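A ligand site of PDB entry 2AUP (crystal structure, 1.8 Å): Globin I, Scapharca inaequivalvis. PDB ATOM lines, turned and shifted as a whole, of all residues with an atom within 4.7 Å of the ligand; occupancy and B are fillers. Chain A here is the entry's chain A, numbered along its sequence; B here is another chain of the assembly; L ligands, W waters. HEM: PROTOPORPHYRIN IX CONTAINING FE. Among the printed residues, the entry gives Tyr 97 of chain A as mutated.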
ATOM      1  N   LEU A  40      37.674 -14.059   7.989  1.00  0.00           N
ATOM      2  CA  LEU A  40      37.786 -12.907   8.880  1.00  0.00           C
ATOM      3  C   LEU A  40      39.048 -13.028   9.728  1.00  0.00           C
ATOM      4  O   LEU A  40      39.830 -12.082   9.845  1.00  0.00           O
ATOM      5  CB  LEU A  40      36.568 -12.827   9.819  1.00  0.00           C
ATOM      6  CG  LEU A  40      36.592 -11.689  10.835  1.00  0.00           C
ATOM      7  CD1 LEU A  40      36.525 -10.358  10.121  1.00  0.00           C
ATOM      8  CD2 LEU A  40      35.432 -11.833  11.806  1.00  0.00           C
ATOM      9  N   THR A  47      41.181  -9.580  15.170  1.00  0.00           N
ATOM     10  CA  THR A  47      39.844  -9.820  15.706  1.00  0.00           C
ATOM     11  C   THR A  47      39.689 -11.100  16.510  1.00  0.00           C
ATOM     12  O   THR A  47      38.722 -11.266  17.260  1.00  0.00           O
ATOM     13  CB  THR A  47      38.791  -9.869  14.572  1.00  0.00           C
ATOM     14  OG1 THR A  47      39.147 -10.896  13.642  1.00  0.00           O
ATOM     15  CG2 THR A  47      38.702  -8.532  13.856  1.00  0.00           C
ATOM     16  N   TYR A  50      38.568 -11.272  20.390  1.00  0.00           N
ATOM     17  CA  TYR A  50      37.175 -11.173  20.818  1.00  0.00           C
ATOM     18  C   TYR A  50      36.504 -12.541  20.877  1.00  0.00           C
ATOM     19  O   TYR A  50      35.460 -12.699  21.513  1.00  0.00           O
ATOM     20  CB  TYR A  50      36.373 -10.301  19.840  1.00  0.00           C
ATOM     21  CG  TYR A  50      36.756  -8.843  19.809  1.00  0.00           C
ATOM     22  CD1 TYR A  50      36.545  -8.015  20.908  1.00  0.00           C
ATOM     23  CD2 TYR A  50      37.282  -8.269  18.652  1.00  0.00           C
ATOM     24  CE1 TYR A  50      36.848  -6.657  20.858  1.00  0.00           C
ATOM     25  CE2 TYR A  50      37.588  -6.919  18.591  1.00  0.00           C
ATOM     26  CZ  TYR A  50      37.361  -6.116  19.698  1.00  0.00           C
ATOM     27  OH  TYR A  50      37.657  -4.768  19.637  1.00  0.00           O
ATOM     28  N   PHE A  51      37.099 -13.514  20.194  1.00  0.00           N
ATOM     29  CA  PHE A  51      36.523 -14.857  20.130  1.00  0.00           C
ATOM     30  C   PHE A  51      37.203 -15.895  21.002  1.00  0.00           C
ATOM     31  O   PHE A  51      37.175 -17.089  20.695  1.00  0.00           O
ATOM     32  CB  PHE A  51      36.525 -15.319  18.665  1.00  0.00           C
ATOM     33  CG  PHE A  51      35.644 -14.488  17.781  1.00  0.00           C
ATOM     34  CD1 PHE A  51      34.298 -14.810  17.641  1.00  0.00           C
ATOM     35  CD2 PHE A  51      36.133 -13.375  17.118  1.00  0.00           C
ATOM     36  CE1 PHE A  51      33.454 -14.036  16.847  1.00  0.00           C
ATOM     37  CE2 PHE A  51      35.307 -12.588  16.336  1.00  0.00           C
ATOM     38  CZ  PHE A  51      33.962 -12.919  16.196  1.00  0.00           C
ATOM     39  N   ARG A  53      36.367 -17.416  23.592  1.00  0.00           N
ATOM     40  CA  ARG A  53      35.506 -18.530  24.004  1.00  0.00           C
ATOM     41  C   ARG A  53      35.482 -19.679  23.007  1.00  0.00           C
ATOM     42  O   ARG A  53      35.308 -20.837  23.395  1.00  0.00           O
ATOM     43  CB  ARG A  53      34.071 -18.044  24.247  1.00  0.00           C
ATOM     44  CG  ARG A  53      33.192 -19.069  24.942  1.00  0.00           C
ATOM     45  CD  ARG A  53      31.751 -18.599  25.023  1.00  0.00           C
ATOM     46  NE  ARG A  53      31.082 -18.713  23.737  1.00  0.00           N
ATOM     47  CZ  ARG A  53      30.766 -19.869  23.165  1.00  0.00           C
ATOM     48  NH1 ARG A  53      31.057 -21.014  23.760  1.00  0.00           N
ATOM     49  NH2 ARG A  53      30.147 -19.873  21.987  1.00  0.00           N
ATOM     50  N   LEU A  54      35.652 -19.363  21.727  1.00  0.00           N
ATOM     51  CA  LEU A  54      35.633 -20.366  20.657  1.00  0.00           C
ATOM     52  C   LEU A  54      36.844 -21.308  20.631  1.00  0.00           C
ATOM     53  O   LEU A  54      36.779 -22.399  20.076  1.00  0.00           O
ATOM     54  CB  LEU A  54      35.481 -19.677  19.297  1.00  0.00           C
ATOM     55  CG  LEU A  54      34.059 -19.357  18.811  1.00  0.00           C
ATOM     56  CD1 LEU A  54      33.216 -18.792  19.933  1.00  0.00           C
ATOM     57  CD2 LEU A  54      34.120 -18.383  17.646  1.00  0.00           C
ATOM     58  N   HIS A  69      28.774 -21.249  16.242  1.00  0.00           N
ATOM     59  CA  HIS A  69      28.696 -19.807  16.104  1.00  0.00           C
ATOM     60  C   HIS A  69      28.438 -19.404  14.654  1.00  0.00           C
ATOM     61  O   HIS A  69      27.593 -18.545  14.366  1.00  0.00           O
ATOM     62  CB  HIS A  69      29.987 -19.140  16.568  1.00  0.00           C
ATOM     63  CG  HIS A  69      30.110 -17.696  16.160  1.00  0.00           C
ATOM     64  ND1 HIS A  69      29.441 -16.708  16.840  1.00  0.00           N
ATOM     65  CD2 HIS A  69      30.791 -17.163  15.120  1.00  0.00           C
ATOM     66  CE1 HIS A  69      29.732 -15.588  16.196  1.00  0.00           C
ATOM     67  NE2 HIS A  69      30.545 -15.804  15.159  1.00  0.00           N
ATOM     68  N   THR A  72      24.913 -20.045  13.464  1.00  0.00           N
ATOM     69  CA  THR A  72      24.045 -19.079  14.112  1.00  0.00           C
ATOM     70  C   THR A  72      24.136 -17.696  13.469  1.00  0.00           C
ATOM     71  O   THR A  72      23.135 -16.980  13.386  1.00  0.00           O
ATOM     72  CB  THR A  72      24.373 -18.966  15.609  1.00  0.00           C
ATOM     73  OG1 THR A  72      24.092 -20.227  16.237  1.00  0.00           O
ATOM     74  CG2 THR A  72      23.540 -17.880  16.265  1.00  0.00           C
ATOM     75  N   LEU A  73      25.324 -17.318  13.022  1.00  0.00           N
ATOM     76  CA  LEU A  73      25.516 -16.024  12.380  1.00  0.00           C
ATOM     77  C   LEU A  73      24.707 -15.963  11.085  1.00  0.00           C
ATOM     78  O   LEU A  73      24.115 -14.935  10.758  1.00  0.00           O
ATOM     79  CB  LEU A  73      27.000 -15.781  12.094  1.00  0.00           C
ATOM     80  CG  LEU A  73      27.413 -14.488  11.375  1.00  0.00           C
ATOM     81  CD1 LEU A  73      28.767 -14.035  11.892  1.00  0.00           C
ATOM     82  CD2 LEU A  73      27.456 -14.705   9.873  1.00  0.00           C
ATOM     83  N   ALA A  76      21.161 -15.082  11.408  1.00  0.00           N
ATOM     84  CA  ALA A  76      20.980 -13.678  11.713  1.00  0.00           C
ATOM     85  C   ALA A  76      20.850 -12.954  10.376  1.00  0.00           C
ATOM     86  O   ALA A  76      20.047 -12.039  10.213  1.00  0.00           O
ATOM     87  CB  ALA A  76      22.187 -13.142  12.488  1.00  0.00           C
ATOM     88  N   LEU A  77      21.662 -13.378   9.399  1.00  0.00           N
ATOM     89  CA  LEU A  77      21.623 -12.788   8.061  1.00  0.00           C
ATOM     90  C   LEU A  77      20.291 -13.160   7.407  1.00  0.00           C
ATOM     91  O   LEU A  77      19.676 -12.340   6.719  1.00  0.00           O
ATOM     92  CB  LEU A  77      22.778 -13.315   7.199  1.00  0.00           C
ATOM     93  CG  LEU A  77      24.009 -12.414   7.039  1.00  0.00           C
ATOM     94  CD1 LEU A  77      24.289 -11.638   8.313  1.00  0.00           C
ATOM     95  CD2 LEU A  77      25.206 -13.275   6.645  1.00  0.00           C
ATOM     96  N   PHE A  80      17.706 -10.851   8.683  1.00  0.00           N
ATOM     97  CA  PHE A  80      17.769  -9.564   7.994  1.00  0.00           C
ATOM     98  C   PHE A  80      17.101  -9.613   6.631  1.00  0.00           C
ATOM     99  O   PHE A  80      16.283  -8.767   6.293  1.00  0.00           O
ATOM    100  CB  PHE A  80      19.230  -9.105   7.816  1.00  0.00           C
ATOM    101  CG  PHE A  80      19.950  -8.796   9.094  1.00  0.00           C
ATOM    102  CD1 PHE A  80      19.244  -8.498  10.261  1.00  0.00           C
ATOM    103  CD2 PHE A  80      21.332  -8.749   9.123  1.00  0.00           C
ATOM    104  CE1 PHE A  80      19.925  -8.163  11.428  1.00  0.00           C
ATOM    105  CE2 PHE A  80      22.023  -8.412  10.291  1.00  0.00           C
ATOM    106  CZ  PHE A  80      21.310  -8.126  11.447  1.00  0.00           C
ATOM    107  N   TYR A  97      20.282  -7.405  17.649  1.00  0.00           N
ATOM    108  CA  TYR A  97      21.586  -8.025  17.493  1.00  0.00           C
ATOM    109  C   TYR A  97      22.716  -7.063  17.872  1.00  0.00           C
ATOM    110  O   TYR A  97      23.799  -7.494  18.263  1.00  0.00           O
ATOM    111  CB  TYR A  97      21.802  -8.482  16.040  1.00  0.00           C
ATOM    112  CG  TYR A  97      20.984  -9.692  15.638  1.00  0.00           C
ATOM    113  CD1 TYR A  97      20.000  -9.588  14.655  1.00  0.00           C
ATOM    114  CD2 TYR A  97      21.207 -10.943  16.214  1.00  0.00           C
ATOM    115  CE1 TYR A  97      19.255 -10.711  14.261  1.00  0.00           C
ATOM    116  CE2 TYR A  97      20.471 -12.065  15.830  1.00  0.00           C
ATOM    117  CZ  TYR A  97      19.503 -11.937  14.849  1.00  0.00           C
ATOM    118  OH  TYR A  97      18.773 -13.036  14.457  1.00  0.00           O
ATOM    119  N   ASN A 100      24.206  -7.072  22.045  1.00  0.00           N
ATOM    120  CA  ASN A 100      25.317  -7.889  22.511  1.00  0.00           C
ATOM    121  C   ASN A 100      26.670  -7.481  21.944  1.00  0.00           C
ATOM    122  O   ASN A 100      27.695  -7.678  22.604  1.00  0.00           O
ATOM    123  CB  ASN A 100      25.074  -9.377  22.218  1.00  0.00           C
ATOM    124  CG  ASN A 100      24.125 -10.028  23.208  1.00  0.00           C
ATOM    125  OD1 ASN A 100      23.874  -9.485  24.291  1.00  0.00           O
ATOM    126  ND2 ASN A 100      23.623 -11.202  22.864  1.00  0.00           N
ATOM    127  N   HIS A 101      26.690  -6.924  20.738  1.00  0.00           N
ATOM    128  CA  HIS A 101      27.946  -6.485  20.156  1.00  0.00           C
ATOM    129  C   HIS A 101      28.404  -5.221  20.872  1.00  0.00           C
ATOM    130  O   HIS A 101      29.592  -4.987  21.060  1.00  0.00           O
ATOM    131  CB  HIS A 101      27.798  -6.241  18.655  1.00  0.00           C
ATOM    132  CG  HIS A 101      27.661  -7.494  17.848  1.00  0.00           C
ATOM    133  ND1 HIS A 101      26.459  -8.118  17.611  1.00  0.00           N
ATOM    134  CD2 HIS A 101      28.606  -8.259  17.234  1.00  0.00           C
ATOM    135  CE1 HIS A 101      26.706  -9.228  16.892  1.00  0.00           C
ATOM    136  NE2 HIS A 101      28.004  -9.365  16.638  1.00  0.00           N
ATOM    137  N   ARG A 104      29.968  -6.152  24.005  1.00  0.00           N
ATOM    138  CA  ARG A 104      31.323  -6.668  23.816  1.00  0.00           C
ATOM    139  C   ARG A 104      32.312  -5.606  23.359  1.00  0.00           C
ATOM    140  O   ARG A 104      33.480  -5.893  23.071  1.00  0.00           O
ATOM    141  CB  ARG A 104      31.300  -7.817  22.809  1.00  0.00           C
ATOM    142  CG  ARG A 104      30.500  -9.002  23.291  1.00  0.00           C
ATOM    143  CD  ARG A 104      30.337 -10.046  22.211  1.00  0.00           C
ATOM    144  NE  ARG A 104      29.394 -11.077  22.642  1.00  0.00           N
ATOM    145  CZ  ARG A 104      28.257 -11.366  22.024  1.00  0.00           C
ATOM    146  NH1 ARG A 104      27.898 -10.701  20.931  1.00  0.00           N
ATOM    147  NH2 ARG A 104      27.467 -12.314  22.507  1.00  0.00           N
ATOM    148  N   ILE A 106      32.306  -3.925  20.569  1.00  0.00           N
ATOM    149  CA  ILE A 106      32.624  -4.063  19.157  1.00  0.00           C
ATOM    150  C   ILE A 106      32.147  -2.764  18.538  1.00  0.00           C
ATOM    151  O   ILE A 106      30.949  -2.454  18.576  1.00  0.00           O
ATOM    152  CB  ILE A 106      31.867  -5.241  18.488  1.00  0.00           C
ATOM    153  CG1 ILE A 106      32.153  -6.546  19.236  1.00  0.00           C
ATOM    154  CG2 ILE A 106      32.292  -5.385  17.032  1.00  0.00           C
ATOM    155  CD1 ILE A 106      33.609  -6.934  19.270  1.00  0.00           C
ATOM    156  N   GLU A 110      35.009  -1.778  13.721  1.00  0.00           N
ATOM    157  CA  GLU A 110      35.369  -3.172  13.948  1.00  0.00           C
ATOM    158  C   GLU A 110      34.385  -4.090  13.228  1.00  0.00           C
ATOM    159  O   GLU A 110      34.773  -5.069  12.583  1.00  0.00           O
ATOM    160  CB  GLU A 110      35.336  -3.476  15.446  1.00  0.00           C
ATOM    161  CG  GLU A 110      36.318  -4.545  15.892  1.00  0.00           C
ATOM    162  CD  GLU A 110      37.693  -3.977  16.176  1.00  0.00           C
ATOM    163  OE1 GLU A 110      37.866  -3.351  17.247  1.00  0.00           O
ATOM    164  OE2 GLU A 110      38.587  -4.152  15.336  1.00  0.00           O
ATOM    165  N   PHE A 111      33.106  -3.760  13.352  1.00  0.00           N
ATOM    166  CA  PHE A 111      32.058  -4.552  12.716  1.00  0.00           C
ATOM    167  C   PHE A 111      32.224  -4.526  11.202  1.00  0.00           C
ATOM    168  O   PHE A 111      31.984  -5.529  10.531  1.00  0.00           O
ATOM    169  CB  PHE A 111      30.698  -3.983  13.117  1.00  0.00           C
ATOM    170  CG  PHE A 111      29.555  -4.922  12.869  1.00  0.00           C
ATOM    171  CD1 PHE A 111      28.850  -4.903  11.668  1.00  0.00           C
ATOM    172  CD2 PHE A 111      29.176  -5.838  13.848  1.00  0.00           C
ATOM    173  CE1 PHE A 111      27.793  -5.773  11.448  1.00  0.00           C
ATOM    174  CE2 PHE A 111      28.117  -6.708  13.639  1.00  0.00           C
ATOM    175  CZ  PHE A 111      27.421  -6.676  12.438  1.00  0.00           C
ATOM    176  N   ILE A 114      33.853  -7.162   8.555  1.00  0.00           N
ATOM    177  CA  ILE A 114      33.177  -8.293   7.913  1.00  0.00           C
ATOM    178  C   ILE A 114      32.936  -8.141   6.413  1.00  0.00           C
ATOM    179  O   ILE A 114      32.683  -9.125   5.711  1.00  0.00           O
ATOM    180  CB  ILE A 114      31.820  -8.583   8.606  1.00  0.00           C
ATOM    181  CG1 ILE A 114      31.372 -10.012   8.294  1.00  0.00           C
ATOM    182  CG2 ILE A 114      30.764  -7.590   8.141  1.00  0.00           C
ATOM    183  CD1 ILE A 114      32.267 -11.055   8.878  1.00  0.00           C
ATOM    184  N   LYS B  96      25.564 -23.285  21.703  1.00  0.00           N
ATOM    185  CA  LYS B  96      25.879 -21.905  21.393  1.00  0.00           C
ATOM    186  C   LYS B  96      24.823 -21.011  22.027  1.00  0.00           C
ATOM    187  O   LYS B  96      25.146 -20.062  22.721  1.00  0.00           O
ATOM    188  CB  LYS B  96      25.925 -21.700  19.871  1.00  0.00           C
ATOM    189  CG  LYS B  96      25.804 -20.246  19.420  1.00  0.00           C
ATOM    190  CD  LYS B  96      26.994 -19.384  19.828  1.00  0.00           C
ATOM    191  CE  LYS B  96      26.649 -17.899  19.717  1.00  0.00           C
ATOM    192  NZ  LYS B  96      27.832 -16.986  19.765  1.00  0.00           N
ATOM    193  N   ASN B 100      24.473 -17.724  26.461  1.00  0.00           N
ATOM    194  CA  ASN B 100      23.893 -16.475  26.947  1.00  0.00           C
ATOM    195  C   ASN B 100      22.813 -16.687  28.010  1.00  0.00           C
ATOM    196  O   ASN B 100      22.640 -15.822  28.872  1.00  0.00           O
ATOM    197  CB  ASN B 100      23.333 -15.627  25.802  1.00  0.00           C
ATOM    198  CG  ASN B 100      24.410 -14.804  25.118  1.00  0.00           C
ATOM    199  OD1 ASN B 100      25.513 -14.611  25.640  1.00  0.00           O
ATOM    200  ND2 ASN B 100      24.090 -14.291  23.931  1.00  0.00           N
HETATM  201  CHA HEM L   1      28.283 -13.186  18.452  1.00  0.00           C
HETATM  202  CHB HEM L   1      25.962 -11.887  14.381  1.00  0.00           C
HETATM  203  CHC HEM L   1      30.015  -9.687  12.865  1.00  0.00           C
HETATM  204  CHD HEM L   1      31.937 -10.244  17.268  1.00  0.00           C
HETATM  205  C1A HEM L   1      27.308 -13.028  17.472  1.00  0.00           C
HETATM  206  C2A HEM L   1      26.024 -13.678  17.470  1.00  0.00           C
HETATM  207  C3A HEM L   1      25.363 -13.274  16.369  1.00  0.00           C
HETATM  208  C4A HEM L   1      26.249 -12.409  15.637  1.00  0.00           C
HETATM  209  CMA HEM L   1      23.943 -13.655  15.991  1.00  0.00           C
HETATM  210  CAA HEM L   1      25.476 -14.713  18.455  1.00  0.00           C
HETATM  211  CBA HEM L   1      24.547 -14.102  19.494  1.00  0.00           C
HETATM  212  CGA HEM L   1      25.291 -13.319  20.554  1.00  0.00           C
HETATM  213  O1A HEM L   1      25.934 -13.945  21.423  1.00  0.00           O
HETATM  214  O2A HEM L   1      25.229 -12.071  20.508  1.00  0.00           O
HETATM  215  C1B HEM L   1      26.859 -11.112  13.635  1.00  0.00           C
HETATM  216  C2B HEM L   1      26.613 -10.699  12.267  1.00  0.00           C
HETATM  217  C3B HEM L   1      27.776 -10.152  11.806  1.00  0.00           C
HETATM  218  C4B HEM L   1      28.720 -10.208  12.919  1.00  0.00           C
HETATM  219  CMB HEM L   1      25.272 -10.774  11.547  1.00  0.00           C
HETATM  220  CAB HEM L   1      28.037  -9.521  10.586  1.00  0.00           C
HETATM  221  CBB HEM L   1      27.376  -9.725   9.317  1.00  0.00           C
HETATM  222  C1C HEM L   1      30.886  -9.635  13.949  1.00  0.00           C
HETATM  223  C2C HEM L   1      32.209  -9.057  13.910  1.00  0.00           C
HETATM  224  C3C HEM L   1      32.744  -9.207  15.146  1.00  0.00           C
HETATM  225  C4C HEM L   1      31.718  -9.828  15.962  1.00  0.00           C
HETATM  226  CMC HEM L   1      32.867  -8.410  12.683  1.00  0.00           C
HETATM  227  CAC HEM L   1      34.057  -8.964  15.582  1.00  0.00           C
HETATM  228  CBC HEM L   1      34.902  -7.875  15.198  1.00  0.00           C
HETATM  229  C1D HEM L   1      31.117 -11.113  17.944  1.00  0.00           C
HETATM  230  C2D HEM L   1      31.532 -11.790  19.160  1.00  0.00           C
HETATM  231  C3D HEM L   1      30.558 -12.680  19.445  1.00  0.00           C
HETATM  232  C4D HEM L   1      29.517 -12.535  18.431  1.00  0.00           C
HETATM  233  CMD HEM L   1      32.813 -11.557  19.964  1.00  0.00           C
HETATM  234  CAD HEM L   1      30.563 -13.630  20.624  1.00  0.00           C
HETATM  235  CBD HEM L   1      31.223 -14.959  20.279  1.00  0.00           C
HETATM  236  CGD HEM L   1      31.113 -15.974  21.399  1.00  0.00           C
HETATM  237  O1D HEM L   1      31.745 -15.758  22.457  1.00  0.00           O
HETATM  238  O2D HEM L   1      30.401 -16.984  21.212  1.00  0.00           O
HETATM  239  NA  HEM L   1      27.444 -12.222  16.334  1.00  0.00           N
HETATM  240  NB  HEM L   1      28.142 -10.773  14.054  1.00  0.00           N
HETATM  241  NC  HEM L   1      30.580 -10.124  15.223  1.00  0.00           N
HETATM  242  ND  HEM L   1      29.897 -11.590  17.483  1.00  0.00           N
HETATM  243 FE   HEM L   1      28.925 -11.011  15.861  1.00  0.00          FE
HETATM  244  O   HOH W   1      23.457 -10.431  19.271  1.00  0.00           O
HETATM  245  O   HOH W   2      34.577 -14.906  22.896  1.00  0.00           O
HETATM  246  O   HOH W   3      30.916 -13.006  14.166  1.00  0.00           O
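A ring nitrogen (NE2) of His 101 binds an iron atom (FE) of the ligand, at 2.0 Å. NH2 of Arg 104 is in salt-bridge range of O1A of the ligand (2.5 Å). The side-chain amino group (NZ) of Lys 96 of chain B is in salt-bridge range of an oxygen (O2D) of the ligand (2.9 Å). O2A of the ligand is in hydrogen-bond range of ND2 of Asn 100 of chain A (3.0 Å). O2D of the ligand is in salt-bridge range of NH2 of Arg 53 (3.0 Å). The side-chain amide nitrogen of Asn 100 of chain B sits at hydrogen-bond distance from an oxygen (O1A) of the ligand (3.1 Å).
The backbone carbonyl oxygen (O) of Tyr 97 is in hydrogen-bond range of a ring nitrogen (ND1) of His 101 (2.8 Å). O of His 101 sits at hydrogen-bond distance from N of Ile 106, at 3.0 Å. O of Asn 100 of chain A sits close to NH1 of Arg 104 (3.5 Å). A ring nitrogen (ND1) of His 69 lies within hydrogen-bond range of the side-chain amino group (NZ) of Lys 96 of chain B (3.3 Å). ND2 of Asn 100 of chain A lies close to ND2 of Asn 100 of chain B, 3.3 Å away. The side-chain hydroxyl of Tyr 50 is in hydrogen-bond range of the side-chain carboxylate of Glu 110, at 2.8 Å.
Residues that only touch the ligand: Tyr 50, Phe 51, Leu 54, His 69, Leu 73, Ala 76, Leu 77, Tyr 97, Glu 110 and Phe 111. Hydrophobic or aromatic side chains within 4 Å of the ligand: Tyr 50, Phe 51, Leu 54, His 69, Leu 73, Ala 76, Leu 77, Tyr 97, His 101 and Phe 111. Of the 22 residues printed, 16 come within 4 Å of the ligand.
Water W1 lies within hydrogen-bond range of an oxygen (O2A) of the ligand (2.7 Å) and the backbone carbonyl oxygen of Tyr 97 (3.1 Å). Water W2 lies within hydrogen-bond range of the backbone carbonyl oxygen (O) of Tyr 50 (2.8 Å), an oxygen (O1D) of the ligand (3.0 Å) and the backbone NH (N) of Arg 53 (3.2 Å).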
